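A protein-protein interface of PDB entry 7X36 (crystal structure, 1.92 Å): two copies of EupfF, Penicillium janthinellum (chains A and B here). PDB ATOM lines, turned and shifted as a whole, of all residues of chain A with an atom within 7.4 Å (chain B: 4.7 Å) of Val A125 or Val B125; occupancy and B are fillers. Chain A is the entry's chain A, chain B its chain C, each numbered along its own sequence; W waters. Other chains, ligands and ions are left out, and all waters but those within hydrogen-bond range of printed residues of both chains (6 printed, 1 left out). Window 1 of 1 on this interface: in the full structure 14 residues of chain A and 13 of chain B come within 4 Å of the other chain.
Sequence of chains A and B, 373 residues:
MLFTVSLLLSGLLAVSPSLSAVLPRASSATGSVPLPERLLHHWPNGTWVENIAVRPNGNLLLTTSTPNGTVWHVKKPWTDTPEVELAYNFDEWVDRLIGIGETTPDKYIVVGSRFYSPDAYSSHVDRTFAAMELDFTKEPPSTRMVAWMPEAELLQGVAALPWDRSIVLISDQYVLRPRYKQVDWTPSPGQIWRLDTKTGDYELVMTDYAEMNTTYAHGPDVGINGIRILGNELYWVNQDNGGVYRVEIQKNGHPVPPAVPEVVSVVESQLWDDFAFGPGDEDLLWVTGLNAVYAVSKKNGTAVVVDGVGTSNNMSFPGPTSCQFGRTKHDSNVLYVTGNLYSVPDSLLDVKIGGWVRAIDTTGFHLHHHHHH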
ATOM      1  N   ASP A  95      14.103  14.810 -15.644  1.00  0.00           N
ATOM      2  CA  ASP A  95      14.533  15.411 -16.898  1.00  0.00           C
ATOM      3  C   ASP A  95      15.087  16.823 -16.699  1.00  0.00           C
ATOM      4  O   ASP A  95      15.910  17.291 -17.493  1.00  0.00           O
ATOM      5  CB  ASP A  95      13.345  15.494 -17.862  1.00  0.00           C
ATOM      6  CG  ASP A  95      12.878  14.083 -18.339  1.00  0.00           C
ATOM      7  OD1 ASP A  95      13.696  13.165 -18.247  1.00  0.00           O
ATOM      8  OD2 ASP A  95      11.717  13.904 -18.777  1.00  0.00           O
ATOM      9  N   SER A 113      11.476  17.432 -12.205  1.00  0.00           N
ATOM     10  CA  SER A 113      10.489  16.446 -12.653  1.00  0.00           C
ATOM     11  C   SER A 113      10.878  15.959 -14.039  1.00  0.00           C
ATOM     12  O   SER A 113      11.869  16.405 -14.624  1.00  0.00           O
ATOM     13  CB  SER A 113       9.086  17.046 -12.722  1.00  0.00           C
ATOM     14  OG  SER A 113       9.065  18.032 -13.739  1.00  0.00           O
ATOM     15  N   ARG A 114      10.052  15.058 -14.581  1.00  0.00           N
ATOM     16  CA  ARG A 114      10.072  14.785 -15.997  1.00  0.00           C
ATOM     17  C   ARG A 114       9.326  15.895 -16.729  1.00  0.00           C
ATOM     18  O   ARG A 114       8.410  16.520 -16.188  1.00  0.00           O
ATOM     19  CB  ARG A 114       9.439  13.406 -16.299  1.00  0.00           C
ATOM     20  CG  ARG A 114      10.081  12.247 -15.538  1.00  0.00           C
ATOM     21  CD  ARG A 114      11.525  11.935 -16.040  1.00  0.00           C
ATOM     22  NE  ARG A 114      12.208  10.978 -15.171  1.00  0.00           N
ATOM     23  CZ  ARG A 114      13.507  10.680 -15.256  1.00  0.00           C
ATOM     24  NH1 ARG A 114      14.261  11.250 -16.172  1.00  0.00           N
ATOM     25  NH2 ARG A 114      14.052   9.813 -14.422  1.00  0.00           N
ATOM     26  N   PHE A 115       9.748  16.157 -17.955  1.00  0.00           N
ATOM     27  CA  PHE A 115       9.097  17.122 -18.824  1.00  0.00           C
ATOM     28  C   PHE A 115       8.814  16.481 -20.174  1.00  0.00           C
ATOM     29  O   PHE A 115       9.550  15.604 -20.622  1.00  0.00           O
ATOM     30  CB  PHE A 115       9.967  18.358 -19.035  1.00  0.00           C
ATOM     31  CG  PHE A 115       9.712  19.470 -18.040  1.00  0.00           C
ATOM     32  CD1 PHE A 115      10.001  19.295 -16.695  1.00  0.00           C
ATOM     33  CD2 PHE A 115       9.191  20.682 -18.464  1.00  0.00           C
ATOM     34  CE1 PHE A 115       9.787  20.343 -15.788  1.00  0.00           C
ATOM     35  CE2 PHE A 115       8.970  21.747 -17.561  1.00  0.00           C
ATOM     36  CZ  PHE A 115       9.261  21.570 -16.224  1.00  0.00           C
ATOM     37  N   TYR A 116       7.748  16.954 -20.830  1.00  0.00           N
ATOM     38  CA  TYR A 116       7.332  16.376 -22.102  1.00  0.00           C
ATOM     39  C   TYR A 116       8.421  16.527 -23.169  1.00  0.00           C
ATOM     40  O   TYR A 116       8.610  15.634 -24.004  1.00  0.00           O
ATOM     41  CB  TYR A 116       5.996  17.003 -22.537  1.00  0.00           C
ATOM     42  CG  TYR A 116       4.793  16.287 -21.918  1.00  0.00           C
ATOM     43  CD1 TYR A 116       4.380  15.046 -22.396  1.00  0.00           C
ATOM     44  CD2 TYR A 116       4.133  16.810 -20.821  1.00  0.00           C
ATOM     45  CE1 TYR A 116       3.312  14.381 -21.838  1.00  0.00           C
ATOM     46  CE2 TYR A 116       3.064  16.162 -20.248  1.00  0.00           C
ATOM     47  CZ  TYR A 116       2.656  14.928 -20.766  1.00  0.00           C
ATOM     48  OH  TYR A 116       1.599  14.259 -20.220  1.00  0.00           O
ATOM     49  N   SER A 117       9.170  17.623 -23.143  1.00  0.00           N
ATOM     50  CA  SER A 117      10.262  17.799 -24.093  1.00  0.00           C
ATOM     51  C   SER A 117      11.233  18.820 -23.528  1.00  0.00           C
ATOM     52  O   SER A 117      10.886  19.564 -22.606  1.00  0.00           O
ATOM     53  CB  SER A 117       9.746  18.253 -25.466  1.00  0.00           C
ATOM     54  OG  SER A 117       9.663  19.662 -25.546  1.00  0.00           O
ATOM     55  N   SER A 122       7.768  23.734 -23.044  1.00  0.00           N
ATOM     56  CA  SER A 122       7.201  22.454 -22.657  1.00  0.00           C
ATOM     57  C   SER A 122       6.677  22.491 -21.230  1.00  0.00           C
ATOM     58  O   SER A 122       7.280  23.101 -20.346  1.00  0.00           O
ATOM     59  CB  SER A 122       8.246  21.343 -22.800  1.00  0.00           C
ATOM     60  OG  SER A 122       7.771  20.133 -22.229  1.00  0.00           O
ATOM     61  N   SER A 123       5.547  21.824 -21.008  1.00  0.00           N
ATOM     62  CA  SER A 123       5.060  21.632 -19.655  1.00  0.00           C
ATOM     63  C   SER A 123       5.820  20.504 -18.986  1.00  0.00           C
ATOM     64  O   SER A 123       6.528  19.722 -19.639  1.00  0.00           O
ATOM     65  CB  SER A 123       3.572  21.320 -19.656  1.00  0.00           C
ATOM     66  OG  SER A 123       2.866  22.320 -20.366  1.00  0.00           O
ATOM     67  N   HIS A 124       5.629  20.387 -17.672  1.00  0.00           N
ATOM     68  CA  HIS A 124       6.121  19.224 -16.948  1.00  0.00           C
ATOM     69  C   HIS A 124       5.186  18.031 -17.185  1.00  0.00           C
ATOM     70  O   HIS A 124       4.114  18.170 -17.774  1.00  0.00           O
ATOM     71  CB  HIS A 124       6.183  19.524 -15.466  1.00  0.00           C
ATOM     72  CG  HIS A 124       4.868  19.965 -14.897  1.00  0.00           C
ATOM     73  ND1 HIS A 124       4.242  21.132 -15.284  1.00  0.00           N
ATOM     74  CD2 HIS A 124       4.060  19.397 -13.969  1.00  0.00           C
ATOM     75  CE1 HIS A 124       3.109  21.267 -14.618  1.00  0.00           C
ATOM     76  NE2 HIS A 124       2.980  20.238 -13.800  1.00  0.00           N
ATOM     77  N   VAL A 125       5.570  16.857 -16.684  1.00  0.00           N
ATOM     78  CA  VAL A 125       4.668  15.707 -16.662  1.00  0.00           C
ATOM     79  C   VAL A 125       4.113  15.555 -15.256  1.00  0.00           C
ATOM     80  O   VAL A 125       4.868  15.411 -14.286  1.00  0.00           O
ATOM     81  CB  VAL A 125       5.361  14.415 -17.126  1.00  0.00           C
ATOM     82  CG1 VAL A 125       4.337  13.294 -17.185  1.00  0.00           C
ATOM     83  CG2 VAL A 125       6.024  14.647 -18.477  1.00  0.00           C
ATOM     84  N   ASP A 126       2.784  15.575 -15.159  1.00  0.00           N
ATOM     85  CA  ASP A 126       2.110  15.599 -13.872  1.00  0.00           C
ATOM     86  C   ASP A 126       2.542  14.424 -13.011  1.00  0.00           C
ATOM     87  O   ASP A 126       2.640  13.271 -13.479  1.00  0.00           O
ATOM     88  CB  ASP A 126       0.580  15.594 -14.082  1.00  0.00           C
ATOM     89  CG  ASP A 126      -0.204  15.959 -12.822  1.00  0.00           C
ATOM     90  OD1 ASP A 126       0.303  16.738 -11.987  1.00  0.00           O
ATOM     91  OD2 ASP A 126      -1.353  15.492 -12.671  1.00  0.00           O
ATOM     92  N   ARG A 127       2.772  14.725 -11.736  1.00  0.00           N
ATOM     93  CA  ARG A 127       3.035  13.782 -10.650  1.00  0.00           C
ATOM     94  C   ARG A 127       4.473  13.285 -10.664  1.00  0.00           C
ATOM     95  O   ARG A 127       4.779  12.366  -9.904  1.00  0.00           O
ATOM     96  CB  ARG A 127       2.091  12.569 -10.646  1.00  0.00           C
ATOM     97  CG  ARG A 127       0.602  12.953 -10.550  1.00  0.00           C
ATOM     98  CD  ARG A 127      -0.297  11.777 -10.301  1.00  0.00           C
ATOM     99  NE  ARG A 127      -0.153  11.214  -8.959  1.00  0.00           N
ATOM    100  CZ  ARG A 127      -0.781  11.677  -7.883  1.00  0.00           C
ATOM    101  NH1 ARG A 127      -1.587  12.718  -7.981  1.00  0.00           N
ATOM    102  NH2 ARG A 127      -0.605  11.102  -6.706  1.00  0.00           N
ATOM    103  N   THR A 128       5.375  13.871 -11.455  1.00  0.00           N
ATOM    104  CA  THR A 128       6.749  13.384 -11.468  1.00  0.00           C
ATOM    105  C   THR A 128       7.731  14.246 -10.667  1.00  0.00           C
ATOM    106  O   THR A 128       8.940  13.983 -10.731  1.00  0.00           O
ATOM    107  CB  THR A 128       7.255  13.249 -12.911  1.00  0.00           C
ATOM    108  OG1 THR A 128       7.232  14.528 -13.558  1.00  0.00           O
ATOM    109  CG2 THR A 128       6.392  12.269 -13.680  1.00  0.00           C
ATOM    110  N   PHE A 129       7.252  15.207  -9.861  1.00  0.00           N
ATOM    111  CA  PHE A 129       8.161  16.088  -9.138  1.00  0.00           C
ATOM    112  C   PHE A 129       8.778  15.381  -7.937  1.00  0.00           C
ATOM    113  O   PHE A 129       8.178  14.485  -7.331  1.00  0.00           O
ATOM    114  CB  PHE A 129       7.459  17.399  -8.714  1.00  0.00           C
ATOM    115  CG  PHE A 129       7.704  18.493  -9.692  1.00  0.00           C
ATOM    116  CD1 PHE A 129       8.876  19.242  -9.619  1.00  0.00           C
ATOM    117  CD2 PHE A 129       6.852  18.670 -10.775  1.00  0.00           C
ATOM    118  CE1 PHE A 129       9.157  20.190 -10.564  1.00  0.00           C
ATOM    119  CE2 PHE A 129       7.132  19.610 -11.733  1.00  0.00           C
ATOM    120  CZ  PHE A 129       8.286  20.391 -11.619  1.00  0.00           C
ATOM    121  N   PRO A 150       4.378  13.447  -5.623  1.00  0.00           N
ATOM    122  CA  PRO A 150       3.451  13.404  -6.760  1.00  0.00           C
ATOM    123  C   PRO A 150       2.273  14.357  -6.631  1.00  0.00           C
ATOM    124  O   PRO A 150       1.686  14.721  -7.665  1.00  0.00           O
ATOM    125  CB  PRO A 150       2.984  11.930  -6.784  1.00  0.00           C
ATOM    126  CG  PRO A 150       3.148  11.462  -5.390  1.00  0.00           C
ATOM    127  CD  PRO A 150       4.389  12.187  -4.862  1.00  0.00           C
ATOM    128  N   ALA A 152       2.390  17.512  -5.605  1.00  0.00           N
ATOM    129  CA  ALA A 152       2.728  18.882  -5.953  1.00  0.00           C
ATOM    130  C   ALA A 152       2.483  19.098  -7.437  1.00  0.00           C
ATOM    131  O   ALA A 152       2.562  18.166  -8.245  1.00  0.00           O
ATOM    132  CB  ALA A 152       4.193  19.182  -5.607  1.00  0.00           C
ATOM    133  N   GLU A 153       2.199  20.345  -7.802  1.00  0.00           N
ATOM    134  CA  GLU A 153       2.041  20.665  -9.218  1.00  0.00           C
ATOM    135  C   GLU A 153       3.400  20.899  -9.877  1.00  0.00           C
ATOM    136  O   GLU A 153       3.838  20.103 -10.706  1.00  0.00           O
ATOM    137  CB  GLU A 153       1.111  21.863  -9.409  1.00  0.00           C
ATOM    138  CG  GLU A 153       0.707  22.017 -10.879  1.00  0.00           C
ATOM    139  CD  GLU A 153       0.029  20.747 -11.442  1.00  0.00           C
ATOM    140  OE1 GLU A 153      -1.105  20.405 -10.993  1.00  0.00           O
ATOM    141  OE2 GLU A 153       0.634  20.101 -12.323  1.00  0.00           O
ATOM    142  N   PRO A 178      -0.934  19.695 -17.036  1.00  0.00           N
ATOM    143  CA  PRO A 178       0.142  19.764 -18.036  1.00  0.00           C
ATOM    144  C   PRO A 178       0.040  18.596 -19.004  1.00  0.00           C
ATOM    145  O   PRO A 178      -0.147  17.458 -18.575  1.00  0.00           O
ATOM    146  CB  PRO A 178       1.416  19.657 -17.194  1.00  0.00           C
ATOM    147  CG  PRO A 178       0.995  18.830 -16.000  1.00  0.00           C
ATOM    148  CD  PRO A 178      -0.462  19.194 -15.736  1.00  0.00           C
ATOM    149  N   ARG A 179       0.208  18.883 -20.306  1.00  0.00           N
ATOM    150  CA  ARG A 179       0.034  17.892 -21.370  1.00  0.00           C
ATOM    151  C   ARG A 179       1.098  18.090 -22.440  1.00  0.00           C
ATOM    152  O   ARG A 179       1.802  19.106 -22.473  1.00  0.00           O
ATOM    153  CB  ARG A 179      -1.355  17.981 -22.033  1.00  0.00           C
ATOM    154  CG  ARG A 179      -2.541  17.797 -21.076  1.00  0.00           C
ATOM    155  CD  ARG A 179      -2.538  16.407 -20.449  1.00  0.00           C
ATOM    156  NE  ARG A 179      -3.722  16.149 -19.628  1.00  0.00           N
ATOM    157  CZ  ARG A 179      -3.772  16.300 -18.306  1.00  0.00           C
ATOM    158  NH1 ARG A 179      -2.696  16.725 -17.628  1.00  0.00           N
ATOM    159  NH2 ARG A 179      -4.918  16.055 -17.663  1.00  0.00           N
ATOM    160  N   TYR A 180       1.177  17.101 -23.338  1.00  0.00           N
ATOM    161  CA  TYR A 180       2.123  17.124 -24.447  1.00  0.00           C
ATOM    162  C   TYR A 180       1.973  18.386 -25.280  1.00  0.00           C
ATOM    163  O   TYR A 180       2.969  18.978 -25.707  1.00  0.00           O
ATOM    164  CB  TYR A 180       1.909  15.879 -25.321  1.00  0.00           C
ATOM    165  CG  TYR A 180       2.518  15.960 -26.695  1.00  0.00           C
ATOM    166  CD1 TYR A 180       3.871  15.729 -26.883  1.00  0.00           C
ATOM    167  CD2 TYR A 180       1.733  16.237 -27.814  1.00  0.00           C
ATOM    168  CE1 TYR A 180       4.443  15.791 -28.137  1.00  0.00           C
ATOM    169  CE2 TYR A 180       2.294  16.300 -29.080  1.00  0.00           C
ATOM    170  CZ  TYR A 180       3.657  16.077 -29.231  1.00  0.00           C
ATOM    171  OH  TYR A 180       4.245  16.117 -30.476  1.00  0.00           O
ATOM    172  N   ARG B 114       1.153   8.532 -18.403  1.00  0.00           N
ATOM    173  CA  ARG B 114       1.555   9.591 -19.317  1.00  0.00           C
ATOM    174  C   ARG B 114       2.618   9.065 -20.272  1.00  0.00           C
ATOM    175  O   ARG B 114       3.389   8.170 -19.932  1.00  0.00           O
ATOM    176  CB  ARG B 114       2.096  10.825 -18.565  1.00  0.00           C
ATOM    177  CG  ARG B 114       1.156  11.375 -17.494  1.00  0.00           C
ATOM    178  CD  ARG B 114      -0.137  11.968 -18.112  1.00  0.00           C
ATOM    179  NE  ARG B 114      -1.115  12.383 -17.097  1.00  0.00           N
ATOM    180  CZ  ARG B 114      -2.326  12.869 -17.381  1.00  0.00           C
ATOM    181  NH1 ARG B 114      -2.702  13.015 -18.645  1.00  0.00           N
ATOM    182  NH2 ARG B 114      -3.173  13.211 -16.402  1.00  0.00           N
ATOM    183  N   PHE B 115       2.655   9.628 -21.483  1.00  0.00           N
ATOM    184  CA  PHE B 115       3.621   9.239 -22.497  1.00  0.00           C
ATOM    185  C   PHE B 115       4.299  10.483 -23.050  1.00  0.00           C
ATOM    186  O   PHE B 115       3.710  11.574 -23.054  1.00  0.00           O
ATOM    187  CB  PHE B 115       2.964   8.437 -23.665  1.00  0.00           C
ATOM    188  CG  PHE B 115       3.019   6.934 -23.490  1.00  0.00           C
ATOM    189  CD1 PHE B 115       2.314   6.309 -22.465  1.00  0.00           C
ATOM    190  CD2 PHE B 115       3.775   6.155 -24.347  1.00  0.00           C
ATOM    191  CE1 PHE B 115       2.362   4.944 -22.302  1.00  0.00           C
ATOM    192  CE2 PHE B 115       3.825   4.775 -24.191  1.00  0.00           C
ATOM    193  CZ  PHE B 115       3.121   4.172 -23.153  1.00  0.00           C
ATOM    194  N   TYR B 116       5.543  10.315 -23.543  1.00  0.00           N
ATOM    195  CA  TYR B 116       6.286  11.490 -24.000  1.00  0.00           C
ATOM    196  C   TYR B 116       5.632  12.129 -25.215  1.00  0.00           C
ATOM    197  O   TYR B 116       5.586  13.362 -25.320  1.00  0.00           O
ATOM    198  CB  TYR B 116       7.748  11.145 -24.279  1.00  0.00           C
ATOM    199  CG  TYR B 116       8.571  11.238 -23.011  1.00  0.00           C
ATOM    200  CD1 TYR B 116       8.958  12.471 -22.496  1.00  0.00           C
ATOM    201  CD2 TYR B 116       8.881  10.109 -22.282  1.00  0.00           C
ATOM    202  CE1 TYR B 116       9.708  12.554 -21.344  1.00  0.00           C
ATOM    203  CE2 TYR B 116       9.614  10.180 -21.123  1.00  0.00           C
ATOM    204  CZ  TYR B 116      10.015  11.421 -20.651  1.00  0.00           C
ATOM    205  OH  TYR B 116      10.741  11.480 -19.501  1.00  0.00           O
ATOM    206  N   SER B 123       8.148   6.481 -25.793  1.00  0.00           N
ATOM    207  CA  SER B 123       8.194   5.779 -24.522  1.00  0.00           C
ATOM    208  C   SER B 123       7.161   6.369 -23.566  1.00  0.00           C
ATOM    209  O   SER B 123       6.641   7.466 -23.783  1.00  0.00           O
ATOM    210  CB  SER B 123       9.593   5.871 -23.912  1.00  0.00           C
ATOM    211  OG  SER B 123      10.532   5.100 -24.682  1.00  0.00           O
ATOM    212  N   HIS B 124       6.841   5.611 -22.514  1.00  0.00           N
ATOM    213  CA  HIS B 124       6.048   6.143 -21.419  1.00  0.00           C
ATOM    214  C   HIS B 124       6.903   7.101 -20.578  1.00  0.00           C
ATOM    215  O   HIS B 124       8.125   7.197 -20.751  1.00  0.00           O
ATOM    216  CB  HIS B 124       5.514   5.011 -20.548  1.00  0.00           C
ATOM    217  CG  HIS B 124       6.581   4.143 -19.951  1.00  0.00           C
ATOM    218  ND1 HIS B 124       7.516   3.468 -20.714  1.00  0.00           N
ATOM    219  CD2 HIS B 124       6.840   3.808 -18.665  1.00  0.00           C
ATOM    220  CE1 HIS B 124       8.314   2.773 -19.921  1.00  0.00           C
ATOM    221  NE2 HIS B 124       7.925   2.959 -18.673  1.00  0.00           N
ATOM    222  N   VAL B 125       6.256   7.812 -19.656  1.00  0.00           N
ATOM    223  CA  VAL B 125       6.959   8.674 -18.703  1.00  0.00           C
ATOM    224  C   VAL B 125       7.039   7.930 -17.379  1.00  0.00           C
ATOM    225  O   VAL B 125       6.015   7.549 -16.804  1.00  0.00           O
ATOM    226  CB  VAL B 125       6.287  10.045 -18.530  1.00  0.00           C
ATOM    227  CG1 VAL B 125       7.092  10.887 -17.493  1.00  0.00           C
ATOM    228  CG2 VAL B 125       6.243  10.779 -19.863  1.00  0.00           C
ATOM    229  N   ASP B 126       8.261   7.715 -16.905  1.00  0.00           N
ATOM    230  CA  ASP B 126       8.487   6.832 -15.773  1.00  0.00           C
ATOM    231  C   ASP B 126       7.697   7.297 -14.556  1.00  0.00           C
ATOM    232  O   ASP B 126       7.595   8.500 -14.277  1.00  0.00           O
ATOM    233  CB  ASP B 126       9.994   6.774 -15.466  1.00  0.00           C
ATOM    234  CG  ASP B 126      10.369   5.666 -14.494  1.00  0.00           C
ATOM    235  OD1 ASP B 126       9.586   4.695 -14.331  1.00  0.00           O
ATOM    236  OD2 ASP B 126      11.463   5.769 -13.875  1.00  0.00           O
ATOM    237  N   ARG B 127       7.145   6.328 -13.822  1.00  0.00           N
ATOM    238  CA  ARG B 127       6.450   6.519 -12.545  1.00  0.00           C
ATOM    239  C   ARG B 127       5.057   7.132 -12.680  1.00  0.00           C
ATOM    240  O   ARG B 127       4.469   7.545 -11.657  1.00  0.00           O
ATOM    241  CB  ARG B 127       7.273   7.375 -11.561  1.00  0.00           C
ATOM    242  CG  ARG B 127       8.644   6.787 -11.211  1.00  0.00           C
ATOM    243  CD  ARG B 127       9.352   7.680 -10.159  1.00  0.00           C
ATOM    244  NE  ARG B 127       8.725   7.560  -8.838  1.00  0.00           N
ATOM    245  CZ  ARG B 127       8.837   6.499  -8.050  1.00  0.00           C
ATOM    246  NH1 ARG B 127       9.567   5.448  -8.426  1.00  0.00           N
ATOM    247  NH2 ARG B 127       8.225   6.474  -6.883  1.00  0.00           N
ATOM    248  N   THR B 128       4.510   7.239 -13.889  1.00  0.00           N
ATOM    249  CA  THR B 128       3.150   7.748 -14.038  1.00  0.00           C
ATOM    250  C   THR B 128       2.088   6.656 -14.262  1.00  0.00           C
ATOM    251  O   THR B 128       0.933   6.992 -14.572  1.00  0.00           O
ATOM    252  CB  THR B 128       3.088   8.761 -15.176  1.00  0.00           C
ATOM    253  OG1 THR B 128       3.447   8.127 -16.399  1.00  0.00           O
ATOM    254  CG2 THR B 128       4.052   9.982 -14.900  1.00  0.00           C
ATOM    255  N   PRO B 178      12.787   4.988 -19.477  1.00  0.00           N
ATOM    256  CA  PRO B 178      12.112   5.692 -20.576  1.00  0.00           C
ATOM    257  C   PRO B 178      12.433   7.178 -20.558  1.00  0.00           C
ATOM    258  O   PRO B 178      12.513   7.788 -19.495  1.00  0.00           O
ATOM    259  CB  PRO B 178      10.623   5.449 -20.285  1.00  0.00           C
ATOM    260  CG  PRO B 178      10.561   5.243 -18.794  1.00  0.00           C
ATOM    261  CD  PRO B 178      11.856   4.537 -18.424  1.00  0.00           C
HETATM  262  O   HOH W   1      -2.101  13.131 -13.522  1.00  0.00           O
HETATM  263  O   HOH W   2       4.469   9.522  -9.735  1.00  0.00           O
HETATM  264  O   HOH W   3      13.534  12.498 -21.149  1.00  0.00           O
HETATM  265  O   HOH W   4       0.178  11.886 -14.223  1.00  0.00           O
HETATM  266  O   HOH W   5      12.324   8.038 -12.674  1.00  0.00           O
HETATM  267  O   HOH W   6      10.022   9.948 -13.126  1.00  0.00           O
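Water W1 lies within hydrogen-bond range of OD2 of Asp A126 (2.6 Å) and NH2 of Arg B114 (3.1 Å). Water W5 bridges OD2 of Asp B126 (2.7 Å) and NH2 of Arg A114 (3.0 Å). Water W2 bridges the backbone carbonyl oxygen of Arg B127 (2.8 Å) and the backbone carbonyl oxygen of Arg A127 (2.9 Å). Water W4 bridges O of Asp A126 (2.9 Å) and NE of Arg B114 (3.2 Å). Water W3 lies within hydrogen-bond range of OD1 of Asp A95 (3.0 Å) and OH of Tyr B116 (3.4 Å). Water W6 lies within hydrogen-bond range of O of Asp B126 (3.1 Å) and NE of Arg A114 (3.2 Å).
O of Arg A114 lies within hydrogen-bond range of N of Val A125. OG1 of Thr A128 sits at hydrogen-bond distance from N of Arg A114 (3.0 Å). The side-chain hydroxyl of Ser A122 lies within hydrogen-bond range of the backbone NH of Tyr A116 (3.5 Å). The backbone NH (N) of Tyr A116 lies within hydrogen-bond range of the backbone carbonyl oxygen (O) of Ser A123. The backbone NH (N) of Val B125 is in hydrogen-bond range of the backbone carbonyl oxygen (O) of Arg B114 (2.9 Å). The side-chain hydroxyl of Thr B128 sits at hydrogen-bond distance from the backbone carbonyl oxygen of Val B125, 2.7 Å away.
Val A125 touches two residues of chain B. Val B125 touches two residues of chain A. Of the printed residues of chain B, Arg A114 touches Tyr B116 and Val B125. Of the printed residues of chain B, Asp A95 touches Tyr B116. Printed residues of chain B within 4 Å of Tyr A116: Arg B114 (3.6 Å), Phe B115 (3.1 Å) and Tyr B116 (3.5 Å). Printed residues of chain B within 4 Å of Tyr A180: Tyr B116 (3.3 Å). Ser A123 touches none of the printed residues of chain B. Pro A150 touches none of the printed residues of chain B. The nearest residue of chain B that does not touch Val A125 is Thr B128 (4.03 Å). The nearest printed residue of chain A that does not touch Tyr B116 is Val A125 (5.1 Å).
Arg A114 touches Tyr B116, and with the chains exchanged Tyr A116 touches Arg B114. Phe A115 touches Tyr B116, and with the chains exchanged Tyr A116 touches Phe B115. Val B125 touches its own counterpart, Val A125. Thr B128 touches its own counterpart, Thr A128.
The side-chain carboxylate of Asp A95 sits at hydrogen-bond distance from the side-chain hydroxyl of Tyr B116 (2.7 Å). NH1 of Arg B114 lies close to NE of Arg A179 (3.4 Å).
Printed residues of chain B that touch a printed residue of chain A: Arg B114, Phe B115, Tyr B116, Val B125 and Thr B128. Hydrophobic or aromatic side chains of chain B within 4 Å of the printed part of chain A: Tyr B116 and Val B125. Along chain B the printed residues that touch a printed residue of chain A span positions 114 to 128. Of the 20 printed residues of chain A, 9 touch a printed residue of chain B. Printed residues of chain A that touch a printed residue of chain B: Asp A95, Arg A114, Phe A115, Tyr A116, Val A125, Asp A126, Thr A128, Arg A179 and Tyr A180. Hydrophobic or aromatic side chains of chain A that line the printed part of chain B: Tyr A116, Val A125 and Tyr A180. Along chain A the printed residues that touch a printed residue of chain B span positions 95 to 180. Among the printed residues, 13 pairs touch across the chains.
Among the printed residues, pairs that only touch across the chains: Tyr A116 with Phe B115, Phe A115 with Tyr B116, Tyr A180 with Tyr B116, Thr A128 with Thr B128, Tyr A116 with Tyr B116, Tyr A116 with Arg B114, Arg A114 with Tyr B116, Val A125 with Arg B114, Arg A114 with Val B125, Val A125 with Val B125 and Asp A126 with Thr B128.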
